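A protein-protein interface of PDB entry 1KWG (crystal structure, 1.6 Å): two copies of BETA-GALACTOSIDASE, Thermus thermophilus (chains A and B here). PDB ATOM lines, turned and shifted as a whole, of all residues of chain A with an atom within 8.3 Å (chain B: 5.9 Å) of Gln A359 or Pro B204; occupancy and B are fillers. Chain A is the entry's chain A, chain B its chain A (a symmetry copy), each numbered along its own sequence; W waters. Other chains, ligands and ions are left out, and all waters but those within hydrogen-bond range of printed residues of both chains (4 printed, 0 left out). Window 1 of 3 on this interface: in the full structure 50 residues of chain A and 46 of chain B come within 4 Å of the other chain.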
ATOM      1  N   PHE A  99       2.107  28.312  19.666  1.00  0.00           N
ATOM      2  CA  PHE A  99       2.188  28.800  18.293  1.00  0.00           C
ATOM      3  C   PHE A  99       3.350  28.058  17.636  1.00  0.00           C
ATOM      4  O   PHE A  99       4.228  27.546  18.332  1.00  0.00           O
ATOM      5  CB  PHE A  99       2.465  30.309  18.338  1.00  0.00           C
ATOM      6  CG  PHE A  99       2.627  30.960  16.991  1.00  0.00           C
ATOM      7  CD1 PHE A  99       3.883  31.064  16.393  1.00  0.00           C
ATOM      8  CD2 PHE A  99       1.527  31.520  16.344  1.00  0.00           C
ATOM      9  CE1 PHE A  99       4.041  31.724  15.172  1.00  0.00           C
ATOM     10  CE2 PHE A  99       1.673  32.178  15.124  1.00  0.00           C
ATOM     11  CZ  PHE A  99       2.930  32.283  14.538  1.00  0.00           C
ATOM     12  N   GLY A 100       3.357  27.987  16.307  1.00  0.00           N
ATOM     13  CA  GLY A 100       4.448  27.308  15.626  1.00  0.00           C
ATOM     14  C   GLY A 100       3.999  26.429  14.475  1.00  0.00           C
ATOM     15  O   GLY A 100       4.744  26.223  13.514  1.00  0.00           O
ATOM     16  N   GLY A 101       2.785  25.900  14.590  1.00  0.00           N
ATOM     17  CA  GLY A 101       2.223  25.058  13.548  1.00  0.00           C
ATOM     18  C   GLY A 101       0.981  25.743  13.016  1.00  0.00           C
ATOM     19  O   GLY A 101       1.065  26.845  12.468  1.00  0.00           O
ATOM     20  N   ARG A 102      -0.175  25.102  13.174  1.00  0.00           N
ATOM     21  CA  ARG A 102      -1.435  25.687  12.724  1.00  0.00           C
ATOM     22  C   ARG A 102      -2.581  25.199  13.600  1.00  0.00           C
ATOM     23  O   ARG A 102      -2.417  24.264  14.383  1.00  0.00           O
ATOM     24  CB  ARG A 102      -1.715  25.336  11.258  1.00  0.00           C
ATOM     25  CG  ARG A 102      -1.923  23.851  10.977  1.00  0.00           C
ATOM     26  CD  ARG A 102      -2.293  23.638   9.515  1.00  0.00           C
ATOM     27  NE  ARG A 102      -2.342  22.223   9.159  1.00  0.00           N
ATOM     28  CZ  ARG A 102      -2.517  21.769   7.923  1.00  0.00           C
ATOM     29  NH1 ARG A 102      -2.664  22.618   6.912  1.00  0.00           N
ATOM     30  NH2 ARG A 102      -2.532  20.461   7.694  1.00  0.00           N
ATOM     31  N   VAL A 318       2.716  12.722  -0.010  1.00  0.00           N
ATOM     32  CA  VAL A 318       2.462  13.709   1.030  1.00  0.00           C
ATOM     33  C   VAL A 318       3.585  13.613   2.061  1.00  0.00           C
ATOM     34  O   VAL A 318       4.508  12.812   1.912  1.00  0.00           O
ATOM     35  CB  VAL A 318       1.078  13.504   1.720  1.00  0.00           C
ATOM     36  CG1 VAL A 318      -0.041  13.691   0.703  1.00  0.00           C
ATOM     37  CG2 VAL A 318       0.997  12.136   2.356  1.00  0.00           C
ATOM     38  N   ASN A 319       3.491  14.415   3.116  1.00  0.00           N
ATOM     39  CA  ASN A 319       4.526  14.474   4.145  1.00  0.00           C
ATOM     40  C   ASN A 319       4.157  13.928   5.515  1.00  0.00           C
ATOM     41  O   ASN A 319       5.037  13.662   6.336  1.00  0.00           O
ATOM     42  CB  ASN A 319       4.900  15.936   4.367  1.00  0.00           C
ATOM     43  CG  ASN A 319       3.709  16.760   4.846  1.00  0.00           C
ATOM     44  OD1 ASN A 319       2.765  17.002   4.089  1.00  0.00           O
ATOM     45  ND2 ASN A 319       3.733  17.170   6.115  1.00  0.00           N
ATOM     46  N   TRP A 320       2.865  13.759   5.758  1.00  0.00           N
ATOM     47  CA  TRP A 320       2.396  13.409   7.091  1.00  0.00           C
ATOM     48  C   TRP A 320       2.104  12.003   7.592  1.00  0.00           C
ATOM     49  O   TRP A 320       1.807  11.840   8.775  1.00  0.00           O
ATOM     50  CB  TRP A 320       1.183  14.282   7.395  1.00  0.00           C
ATOM     51  CG  TRP A 320       0.171  14.284   6.295  1.00  0.00           C
ATOM     52  CD1 TRP A 320       0.050  15.202   5.290  1.00  0.00           C
ATOM     53  CD2 TRP A 320      -0.872  13.328   6.094  1.00  0.00           C
ATOM     54  NE1 TRP A 320      -1.012  14.878   4.479  1.00  0.00           N
ATOM     55  CE2 TRP A 320      -1.596  13.731   4.949  1.00  0.00           C
ATOM     56  CE3 TRP A 320      -1.269  12.167   6.773  1.00  0.00           C
ATOM     57  CZ2 TRP A 320      -2.698  13.015   4.468  1.00  0.00           C
ATOM     58  CZ3 TRP A 320      -2.367  11.454   6.296  1.00  0.00           C
ATOM     59  CH2 TRP A 320      -3.067  11.883   5.155  1.00  0.00           C
ATOM     60  N   ALA A 355       6.198  23.470  -2.057  1.00  0.00           N
ATOM     61  CA  ALA A 355       6.930  24.497  -1.319  1.00  0.00           C
ATOM     62  C   ALA A 355       8.307  23.957  -0.937  1.00  0.00           C
ATOM     63  O   ALA A 355       8.443  22.791  -0.559  1.00  0.00           O
ATOM     64  CB  ALA A 355       6.165  24.890  -0.068  1.00  0.00           C
ATOM     65  N   PRO A 356       9.353  24.795  -1.042  1.00  0.00           N
ATOM     66  CA  PRO A 356      10.704  24.350  -0.695  1.00  0.00           C
ATOM     67  C   PRO A 356      11.068  24.597   0.768  1.00  0.00           C
ATOM     68  O   PRO A 356      12.158  24.243   1.210  1.00  0.00           O
ATOM     69  CB  PRO A 356      11.575  25.162  -1.641  1.00  0.00           C
ATOM     70  CG  PRO A 356      10.863  26.478  -1.655  1.00  0.00           C
ATOM     71  CD  PRO A 356       9.398  26.074  -1.777  1.00  0.00           C
ATOM     72  N   PHE A 357      10.152  25.200   1.515  1.00  0.00           N
ATOM     73  CA  PHE A 357      10.404  25.506   2.918  1.00  0.00           C
ATOM     74  C   PHE A 357       9.280  25.065   3.844  1.00  0.00           C
ATOM     75  O   PHE A 357       8.194  24.706   3.395  1.00  0.00           O
ATOM     76  CB  PHE A 357      10.622  27.019   3.084  1.00  0.00           C
ATOM     77  CG  PHE A 357       9.596  27.866   2.374  1.00  0.00           C
ATOM     78  CD1 PHE A 357       9.940  28.582   1.231  1.00  0.00           C
ATOM     79  CD2 PHE A 357       8.285  27.934   2.837  1.00  0.00           C
ATOM     80  CE1 PHE A 357       8.992  29.355   0.556  1.00  0.00           C
ATOM     81  CE2 PHE A 357       7.329  28.703   2.170  1.00  0.00           C
ATOM     82  CZ  PHE A 357       7.683  29.414   1.028  1.00  0.00           C
ATOM     83  N   ALA A 358       9.568  25.096   5.142  1.00  0.00           N
ATOM     84  CA  ALA A 358       8.608  24.772   6.197  1.00  0.00           C
ATOM     85  C   ALA A 358       8.114  23.331   6.310  1.00  0.00           C
ATOM     86  O   ALA A 358       8.620  22.428   5.646  1.00  0.00           O
ATOM     87  CB  ALA A 358       7.416  25.732   6.120  1.00  0.00           C
ATOM     88  N   GLN A 359       7.112  23.149   7.167  1.00  0.00           N
ATOM     89  CA  GLN A 359       6.532  21.844   7.486  1.00  0.00           C
ATOM     90  C   GLN A 359       6.170  20.897   6.361  1.00  0.00           C
ATOM     91  O   GLN A 359       6.387  19.690   6.480  1.00  0.00           O
ATOM     92  CB  GLN A 359       5.292  22.018   8.373  1.00  0.00           C
ATOM     93  CG  GLN A 359       5.602  22.430   9.804  1.00  0.00           C
ATOM     94  CD  GLN A 359       5.544  23.931  10.028  1.00  0.00           C
ATOM     95  OE1 GLN A 359       5.897  24.723   9.154  1.00  0.00           O
ATOM     96  NE2 GLN A 359       5.115  24.327  11.222  1.00  0.00           N
ATOM     97  N   GLU A 360       5.608  21.428   5.283  1.00  0.00           N
ATOM     98  CA  GLU A 360       5.186  20.578   4.180  1.00  0.00           C
ATOM     99  C   GLU A 360       6.079  20.620   2.950  1.00  0.00           C
ATOM    100  O   GLU A 360       5.613  20.413   1.828  1.00  0.00           O
ATOM    101  CB  GLU A 360       3.740  20.924   3.801  1.00  0.00           C
ATOM    102  CG  GLU A 360       2.754  20.584   4.914  1.00  0.00           C
ATOM    103  CD  GLU A 360       1.312  20.906   4.576  1.00  0.00           C
ATOM    104  OE1 GLU A 360       0.424  20.416   5.305  1.00  0.00           O
ATOM    105  OE2 GLU A 360       1.057  21.650   3.606  1.00  0.00           O
ATOM    106  N   GLN A 361       7.370  20.859   3.151  1.00  0.00           N
ATOM    107  CA  GLN A 361       8.281  20.907   2.018  1.00  0.00           C
ATOM    108  C   GLN A 361       8.353  19.566   1.277  1.00  0.00           C
ATOM    109  O   GLN A 361       8.751  19.524   0.115  1.00  0.00           O
ATOM    110  CB  GLN A 361       9.678  21.347   2.468  1.00  0.00           C
ATOM    111  CG  GLN A 361      10.364  20.427   3.460  1.00  0.00           C
ATOM    112  CD  GLN A 361      11.666  21.014   3.968  1.00  0.00           C
ATOM    113  OE1 GLN A 361      12.752  20.487   3.710  1.00  0.00           O
ATOM    114  NE2 GLN A 361      11.563  22.123   4.691  1.00  0.00           N
ATOM    115  N   MET A 362       7.964  18.478   1.939  1.00  0.00           N
ATOM    116  CA  MET A 362       7.990  17.166   1.290  1.00  0.00           C
ATOM    117  C   MET A 362       6.632  16.790   0.686  1.00  0.00           C
ATOM    118  O   MET A 362       6.445  15.668   0.204  1.00  0.00           O
ATOM    119  CB  MET A 362       8.445  16.082   2.274  1.00  0.00           C
ATOM    120  CG  MET A 362       9.833  16.327   2.867  1.00  0.00           C
ATOM    121  SD  MET A 362      11.143  16.532   1.628  1.00  0.00           S
ATOM    122  CE  MET A 362      11.729  14.825   1.468  1.00  0.00           C
ATOM    123  N   HIS A 363       5.685  17.726   0.711  1.00  0.00           N
ATOM    124  CA  HIS A 363       4.362  17.486   0.134  1.00  0.00           C
ATOM    125  C   HIS A 363       4.411  17.908  -1.335  1.00  0.00           C
ATOM    126  O   HIS A 363       4.566  19.086  -1.653  1.00  0.00           O
ATOM    127  CB  HIS A 363       3.297  18.301   0.877  1.00  0.00           C
ATOM    128  CG  HIS A 363       1.889  17.902   0.551  1.00  0.00           C
ATOM    129  ND1 HIS A 363       1.385  17.917  -0.733  1.00  0.00           N
ATOM    130  CD2 HIS A 363       0.874  17.493   1.348  1.00  0.00           C
ATOM    131  CE1 HIS A 363       0.119  17.536  -0.712  1.00  0.00           C
ATOM    132  NE2 HIS A 363      -0.216  17.275   0.539  1.00  0.00           N
ATOM    133  N   PHE B 181       4.552  30.589   5.486  1.00  0.00           N
ATOM    134  CA  PHE B 181       3.813  29.336   5.600  1.00  0.00           C
ATOM    135  C   PHE B 181       3.045  29.267   6.922  1.00  0.00           C
ATOM    136  O   PHE B 181       3.615  29.466   7.998  1.00  0.00           O
ATOM    137  CB  PHE B 181       4.783  28.156   5.480  1.00  0.00           C
ATOM    138  CG  PHE B 181       4.106  26.824   5.349  1.00  0.00           C
ATOM    139  CD1 PHE B 181       4.010  25.969   6.440  1.00  0.00           C
ATOM    140  CD2 PHE B 181       3.561  26.427   4.133  1.00  0.00           C
ATOM    141  CE1 PHE B 181       3.379  24.730   6.318  1.00  0.00           C
ATOM    142  CE2 PHE B 181       2.927  25.193   4.002  1.00  0.00           C
ATOM    143  CZ  PHE B 181       2.838  24.344   5.097  1.00  0.00           C
ATOM    144  N   TRP B 182       1.750  28.973   6.824  1.00  0.00           N
ATOM    145  CA  TRP B 182       0.864  28.890   7.984  1.00  0.00           C
ATOM    146  C   TRP B 182       0.919  30.142   8.857  1.00  0.00           C
ATOM    147  O   TRP B 182       0.724  30.068  10.066  1.00  0.00           O
ATOM    148  CB  TRP B 182       1.184  27.657   8.836  1.00  0.00           C
ATOM    149  CG  TRP B 182       0.811  26.344   8.194  1.00  0.00           C
ATOM    150  CD1 TRP B 182       0.114  26.160   7.026  1.00  0.00           C
ATOM    151  CD2 TRP B 182       1.136  25.034   8.674  1.00  0.00           C
ATOM    152  NE1 TRP B 182      -0.006  24.814   6.752  1.00  0.00           N
ATOM    153  CE2 TRP B 182       0.614  24.103   7.746  1.00  0.00           C
ATOM    154  CE3 TRP B 182       1.826  24.556   9.798  1.00  0.00           C
ATOM    155  CZ2 TRP B 182       0.761  22.720   7.911  1.00  0.00           C
ATOM    156  CZ3 TRP B 182       1.971  23.184   9.960  1.00  0.00           C
ATOM    157  CH2 TRP B 182       1.440  22.283   9.018  1.00  0.00           C
ATOM    158  N   GLN B 184       3.315  31.984  10.075  1.00  0.00           N
ATOM    159  CA  GLN B 184       4.260  31.907  11.185  1.00  0.00           C
ATOM    160  C   GLN B 184       5.087  33.184  11.354  1.00  0.00           C
ATOM    161  O   GLN B 184       5.842  33.301  12.313  1.00  0.00           O
ATOM    162  CB  GLN B 184       5.222  30.735  10.974  1.00  0.00           C
ATOM    163  CG  GLN B 184       4.592  29.360  11.119  1.00  0.00           C
ATOM    164  CD  GLN B 184       5.518  28.249  10.649  1.00  0.00           C
ATOM    165  OE1 GLN B 184       6.664  28.150  11.089  1.00  0.00           O
ATOM    166  NE2 GLN B 184       5.022  27.409   9.752  1.00  0.00           N
ATOM    167  N   GLU B 201       2.873  19.861  13.436  1.00  0.00           N
ATOM    168  CA  GLU B 201       4.321  19.807  13.593  1.00  0.00           C
ATOM    169  C   GLU B 201       4.998  21.176  13.561  1.00  0.00           C
ATOM    170  O   GLU B 201       4.518  22.104  12.911  1.00  0.00           O
ATOM    171  CB  GLU B 201       4.920  18.924  12.493  1.00  0.00           C
ATOM    172  CG  GLU B 201       4.395  17.486  12.468  1.00  0.00           C
ATOM    173  CD  GLU B 201       2.873  17.402  12.408  1.00  0.00           C
ATOM    174  OE1 GLU B 201       2.266  18.045  11.523  1.00  0.00           O
ATOM    175  OE2 GLU B 201       2.283  16.685  13.248  1.00  0.00           O
ATOM    176  N   PRO B 202       6.119  21.320  14.287  1.00  0.00           N
ATOM    177  CA  PRO B 202       6.834  22.596  14.295  1.00  0.00           C
ATOM    178  C   PRO B 202       7.587  22.735  12.971  1.00  0.00           C
ATOM    179  O   PRO B 202       7.789  21.750  12.254  1.00  0.00           O
ATOM    180  CB  PRO B 202       7.775  22.454  15.489  1.00  0.00           C
ATOM    181  CG  PRO B 202       8.091  20.988  15.479  1.00  0.00           C
ATOM    182  CD  PRO B 202       6.736  20.365  15.224  1.00  0.00           C
ATOM    183  N   ASN B 203       7.982  23.958  12.640  1.00  0.00           N
ATOM    184  CA  ASN B 203       8.713  24.218  11.404  1.00  0.00           C
ATOM    185  C   ASN B 203      10.064  23.500  11.484  1.00  0.00           C
ATOM    186  O   ASN B 203      10.792  23.645  12.464  1.00  0.00           O
ATOM    187  CB  ASN B 203       8.934  25.728  11.263  1.00  0.00           C
ATOM    188  CG  ASN B 203       9.479  26.122   9.905  1.00  0.00           C
ATOM    189  OD1 ASN B 203      10.355  25.457   9.351  1.00  0.00           O
ATOM    190  ND2 ASN B 203       8.976  27.226   9.369  1.00  0.00           N
ATOM    191  N   PRO B 204      10.423  22.713  10.457  1.00  0.00           N
ATOM    192  CA  PRO B 204      11.713  22.016  10.516  1.00  0.00           C
ATOM    193  C   PRO B 204      12.934  22.921  10.693  1.00  0.00           C
ATOM    194  O   PRO B 204      13.889  22.548  11.384  1.00  0.00           O
ATOM    195  CB  PRO B 204      11.743  21.229   9.202  1.00  0.00           C
ATOM    196  CG  PRO B 204      10.860  22.035   8.287  1.00  0.00           C
ATOM    197  CD  PRO B 204       9.720  22.423   9.196  1.00  0.00           C
ATOM    198  N   SER B 205      12.910  24.100  10.077  1.00  0.00           N
ATOM    199  CA  SER B 205      14.022  25.046  10.195  1.00  0.00           C
ATOM    200  C   SER B 205      14.110  25.515  11.643  1.00  0.00           C
ATOM    201  O   SER B 205      15.195  25.697  12.193  1.00  0.00           O
ATOM    202  CB  SER B 205      13.790  26.264   9.295  1.00  0.00           C
ATOM    203  OG  SER B 205      13.600  25.884   7.945  1.00  0.00           O
ATOM    204  N   HIS B 206      12.939  25.712  12.234  1.00  0.00           N
ATOM    205  CA  HIS B 206      12.781  26.157  13.615  1.00  0.00           C
ATOM    206  C   HIS B 206      13.332  25.096  14.575  1.00  0.00           C
ATOM    207  O   HIS B 206      14.107  25.403  15.486  1.00  0.00           O
ATOM    208  CB  HIS B 206      11.285  26.395  13.864  1.00  0.00           C
ATOM    209  CG  HIS B 206      10.950  26.962  15.210  1.00  0.00           C
ATOM    210  ND1 HIS B 206       9.658  27.287  15.567  1.00  0.00           N
ATOM    211  CD2 HIS B 206      11.723  27.268  16.278  1.00  0.00           C
ATOM    212  CE1 HIS B 206       9.650  27.770  16.795  1.00  0.00           C
ATOM    213  NE2 HIS B 206      10.891  27.769  17.252  1.00  0.00           N
ATOM    214  N   LEU B 207      12.937  23.846  14.357  1.00  0.00           N
ATOM    215  CA  LEU B 207      13.388  22.751  15.206  1.00  0.00           C
ATOM    216  C   LEU B 207      14.883  22.484  15.047  1.00  0.00           C
ATOM    217  O   LEU B 207      15.579  22.250  16.037  1.00  0.00           O
ATOM    218  CB  LEU B 207      12.579  21.479  14.902  1.00  0.00           C
ATOM    219  CG  LEU B 207      12.756  20.308  15.872  1.00  0.00           C
ATOM    220  CD1 LEU B 207      12.475  20.768  17.297  1.00  0.00           C
ATOM    221  CD2 LEU B 207      11.808  19.174  15.493  1.00  0.00           C
ATOM    222  N   LEU B 208      15.382  22.524  13.813  1.00  0.00           N
ATOM    223  CA  LEU B 208      16.806  22.298  13.584  1.00  0.00           C
ATOM    224  C   LEU B 208      17.630  23.386  14.274  1.00  0.00           C
ATOM    225  O   LEU B 208      18.656  23.097  14.886  1.00  0.00           O
ATOM    226  CB  LEU B 208      17.132  22.284  12.086  1.00  0.00           C
ATOM    227  CG  LEU B 208      18.626  22.194  11.752  1.00  0.00           C
ATOM    228  CD1 LEU B 208      19.205  20.889  12.293  1.00  0.00           C
ATOM    229  CD2 LEU B 208      18.820  22.283  10.246  1.00  0.00           C
ATOM    230  N   ASP B 209      17.196  24.638  14.168  1.00  0.00           N
ATOM    231  CA  ASP B 209      17.938  25.712  14.817  1.00  0.00           C
ATOM    232  C   ASP B 209      17.926  25.517  16.330  1.00  0.00           C
ATOM    233  O   ASP B 209      18.908  25.820  17.011  1.00  0.00           O
ATOM    234  CB  ASP B 209      17.359  27.079  14.451  1.00  0.00           C
ATOM    235  CG  ASP B 209      17.910  27.611  13.140  1.00  0.00           C
ATOM    236  OD1 ASP B 209      18.827  26.978  12.568  1.00  0.00           O
ATOM    237  OD2 ASP B 209      17.436  28.669  12.683  1.00  0.00           O
ATOM    238  N   VAL B 414      14.392  15.502  12.729  1.00  0.00           N
ATOM    239  CA  VAL B 414      13.336  16.478  12.490  1.00  0.00           C
ATOM    240  C   VAL B 414      12.402  16.051  11.364  1.00  0.00           C
ATOM    241  O   VAL B 414      11.180  16.163  11.478  1.00  0.00           O
ATOM    242  CB  VAL B 414      13.935  17.852  12.116  1.00  0.00           C
ATOM    243  CG1 VAL B 414      12.835  18.805  11.671  1.00  0.00           C
ATOM    244  CG2 VAL B 414      14.684  18.427  13.305  1.00  0.00           C
ATOM    245  N   GLN B 415      12.985  15.554  10.279  1.00  0.00           N
ATOM    246  CA  GLN B 415      12.203  15.160   9.117  1.00  0.00           C
ATOM    247  C   GLN B 415      12.531  13.759   8.608  1.00  0.00           C
ATOM    248  O   GLN B 415      13.236  13.595   7.611  1.00  0.00           O
ATOM    249  CB  GLN B 415      12.434  16.178   7.998  1.00  0.00           C
ATOM    250  CG  GLN B 415      11.520  16.033   6.799  1.00  0.00           C
ATOM    251  CD  GLN B 415      12.014  16.833   5.616  1.00  0.00           C
ATOM    252  OE1 GLN B 415      12.818  16.351   4.816  1.00  0.00           O
ATOM    253  NE2 GLN B 415      11.556  18.070   5.511  1.00  0.00           N
ATOM    254  N   PHE B 492      17.401  24.473   6.072  1.00  0.00           N
ATOM    255  CA  PHE B 492      16.395  23.412   5.990  1.00  0.00           C
ATOM    256  C   PHE B 492      15.347  23.656   4.906  1.00  0.00           C
ATOM    257  O   PHE B 492      14.143  23.527   5.139  1.00  0.00           O
ATOM    258  CB  PHE B 492      15.709  23.220   7.353  1.00  0.00           C
ATOM    259  CG  PHE B 492      15.390  21.778   7.684  1.00  0.00           C
ATOM    260  CD1 PHE B 492      15.614  21.284   8.967  1.00  0.00           C
ATOM    261  CD2 PHE B 492      14.874  20.916   6.717  1.00  0.00           C
ATOM    262  CE1 PHE B 492      15.335  19.954   9.284  1.00  0.00           C
ATOM    263  CE2 PHE B 492      14.591  19.584   7.022  1.00  0.00           C
ATOM    264  CZ  PHE B 492      14.823  19.101   8.306  1.00  0.00           C
HETATM  265  O   HOH W   1      -0.613  23.783   3.988  1.00  0.00           O
HETATM  266  O   HOH W   2       7.353  26.047  14.375  1.00  0.00           O
HETATM  267  O   HOH W   3      12.240  25.625   5.736  1.00  0.00           O
HETATM  268  O   HOH W   4       9.455  18.972   7.415  1.00  0.00           O
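The side-chain amide oxygen (OE1) of Gln A359 sits at hydrogen-bond distance from the side-chain amide nitrogen (NE2) of Gln B184 (2.9 Å). NE2 of Gln A359 is in hydrogen-bond range of O of Glu B201. N of Asn B203 sits close to NE2 of Gln A359 (3.2 Å). The side-chain amide oxygen (OE1) of Gln A361 lies within hydrogen-bond range of the side-chain amide nitrogen (NE2) of Gln B415 (3.2 Å). NE2 of Gln A361 is in hydrogen-bond range of O of Phe B492 (3.0 Å). OE1 of Gln B415 sits close to SD of Met A362 (3.6 Å). The indole nitrogen of Trp B182 lies close to the guanidinium group of Arg A102 (3.5 Å).
The side-chain amide nitrogen of Gln A359 lies within hydrogen-bond range of the backbone carbonyl oxygen of Gly A100, at 3.0 Å. NH2 of Arg A102 lies within salt-bridge range of OE1 of Glu A360 (3.8 Å). The side-chain amide nitrogen (NE2) of Gln A361 lies within hydrogen-bond range of the backbone carbonyl oxygen (O) of Ala A358. NE2 of Gln B184 lies within hydrogen-bond range of O of Phe B181 (3.0 Å). The side-chain amide nitrogen of Asn B203 lies within hydrogen-bond range of the side-chain amide oxygen of Gln B184, at 3.0 Å. The side-chain amide oxygen of Asn B203 is in hydrogen-bond range of the backbone NH of Ser B205, 3.0 Å away.
Among the printed residues, pairs that only touch across the chains: Phe A99 with Gln B184 (3.6 Å), Gly A100 with Gln B184 (3.6 Å), Gly A101 with Trp B182 (3.5 Å), Gly A101 with Glu B201 (3.8 Å), Ala A358 with Phe B181 (3.4 Å), Ala A358 with Asn B203 (3.7 Å), Ala A358 with Pro B204 (3.4 Å), Gln A359 with Phe B181 (3.5 Å), Gln A359 with Trp B182 (3.6 Å), Gln A359 with Pro B202 (3.4 Å), Gln A359 with Pro B204 (3.4 Å), Glu A360 with Phe B181 (3.6 Å), Glu A360 with Trp B182 (3.5 Å) and Gln A361 with Pro B204 (3.7 Å).
Of the printed residues of chain B, Gln A359 touches Phe B181, Trp B182, Gln B184, Glu B201, Pro B202, Asn B203 and Pro B204. Of chain A, only Ala A358 (3.4 Å), Gln A359 (3.4 Å) and Gln A361 (3.7 Å) come within 4 Å of Pro B204. Of chain A, only Ala A358 and Gln A359 come within 4 Å of Asn B203. Of the printed residues of chain A, Gln B415 touches Gln A361 and Met A362. Of the printed residues of chain B, Gln A361 touches Pro B204 (3.7 Å), Gln B415 (3.2 Å) and Phe B492 (3.0 Å). Of the printed residues of chain B, Gly A101 touches Trp B182 (3.5 Å) and Glu B201 (3.8 Å). Printed residues of chain B within 4 Å of Ala A358: Phe B181, Asn B203 and Pro B204. Phe A357 touches none of the printed residues of chain B. Leu B207 touches none of the printed residues of chain A. The nearest residue of chain B that does not touch Gln A359 is Gln B415 (5.5 Å). The nearest residue of chain A that does not touch Pro B204 is Phe A357 (5.6 Å).
Of the 16 printed residues of chain A, 9 touch a printed residue of chain B. Of the 15 printed residues of chain B, 9 touch a printed residue of chain A. Among the printed residues, no Asp or Glu carboxylate lies within 4 Å of a Lys or Arg side-chain nitrogen of the other chain.
No position is printed for both chains. Of the 21 pairs that touch across the chains among the printed residues, none has its exchanged pair printed and touching as well.
Water W3 lies within hydrogen-bond range of OG of Ser B205 (2.6 Å), N of Ala A358 (2.8 Å) and O of Phe B492 (2.9 Å). Water W1 bridges OE2 of Glu A360 (2.7 Å) and NE1 of Trp B182 (3.0 Å). Water W2 lies within hydrogen-bond range of the backbone carbonyl oxygen (O) of Gly A100 (2.8 Å), the backbone NH (N) of Asn B203 (2.8 Å) and a ring nitrogen (ND1) of His B206 (2.9 Å). Water W4 lies within hydrogen-bond range of NE2 of Gln B415 (3.0 Å) and O of Gln A359 (3.3 Å).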
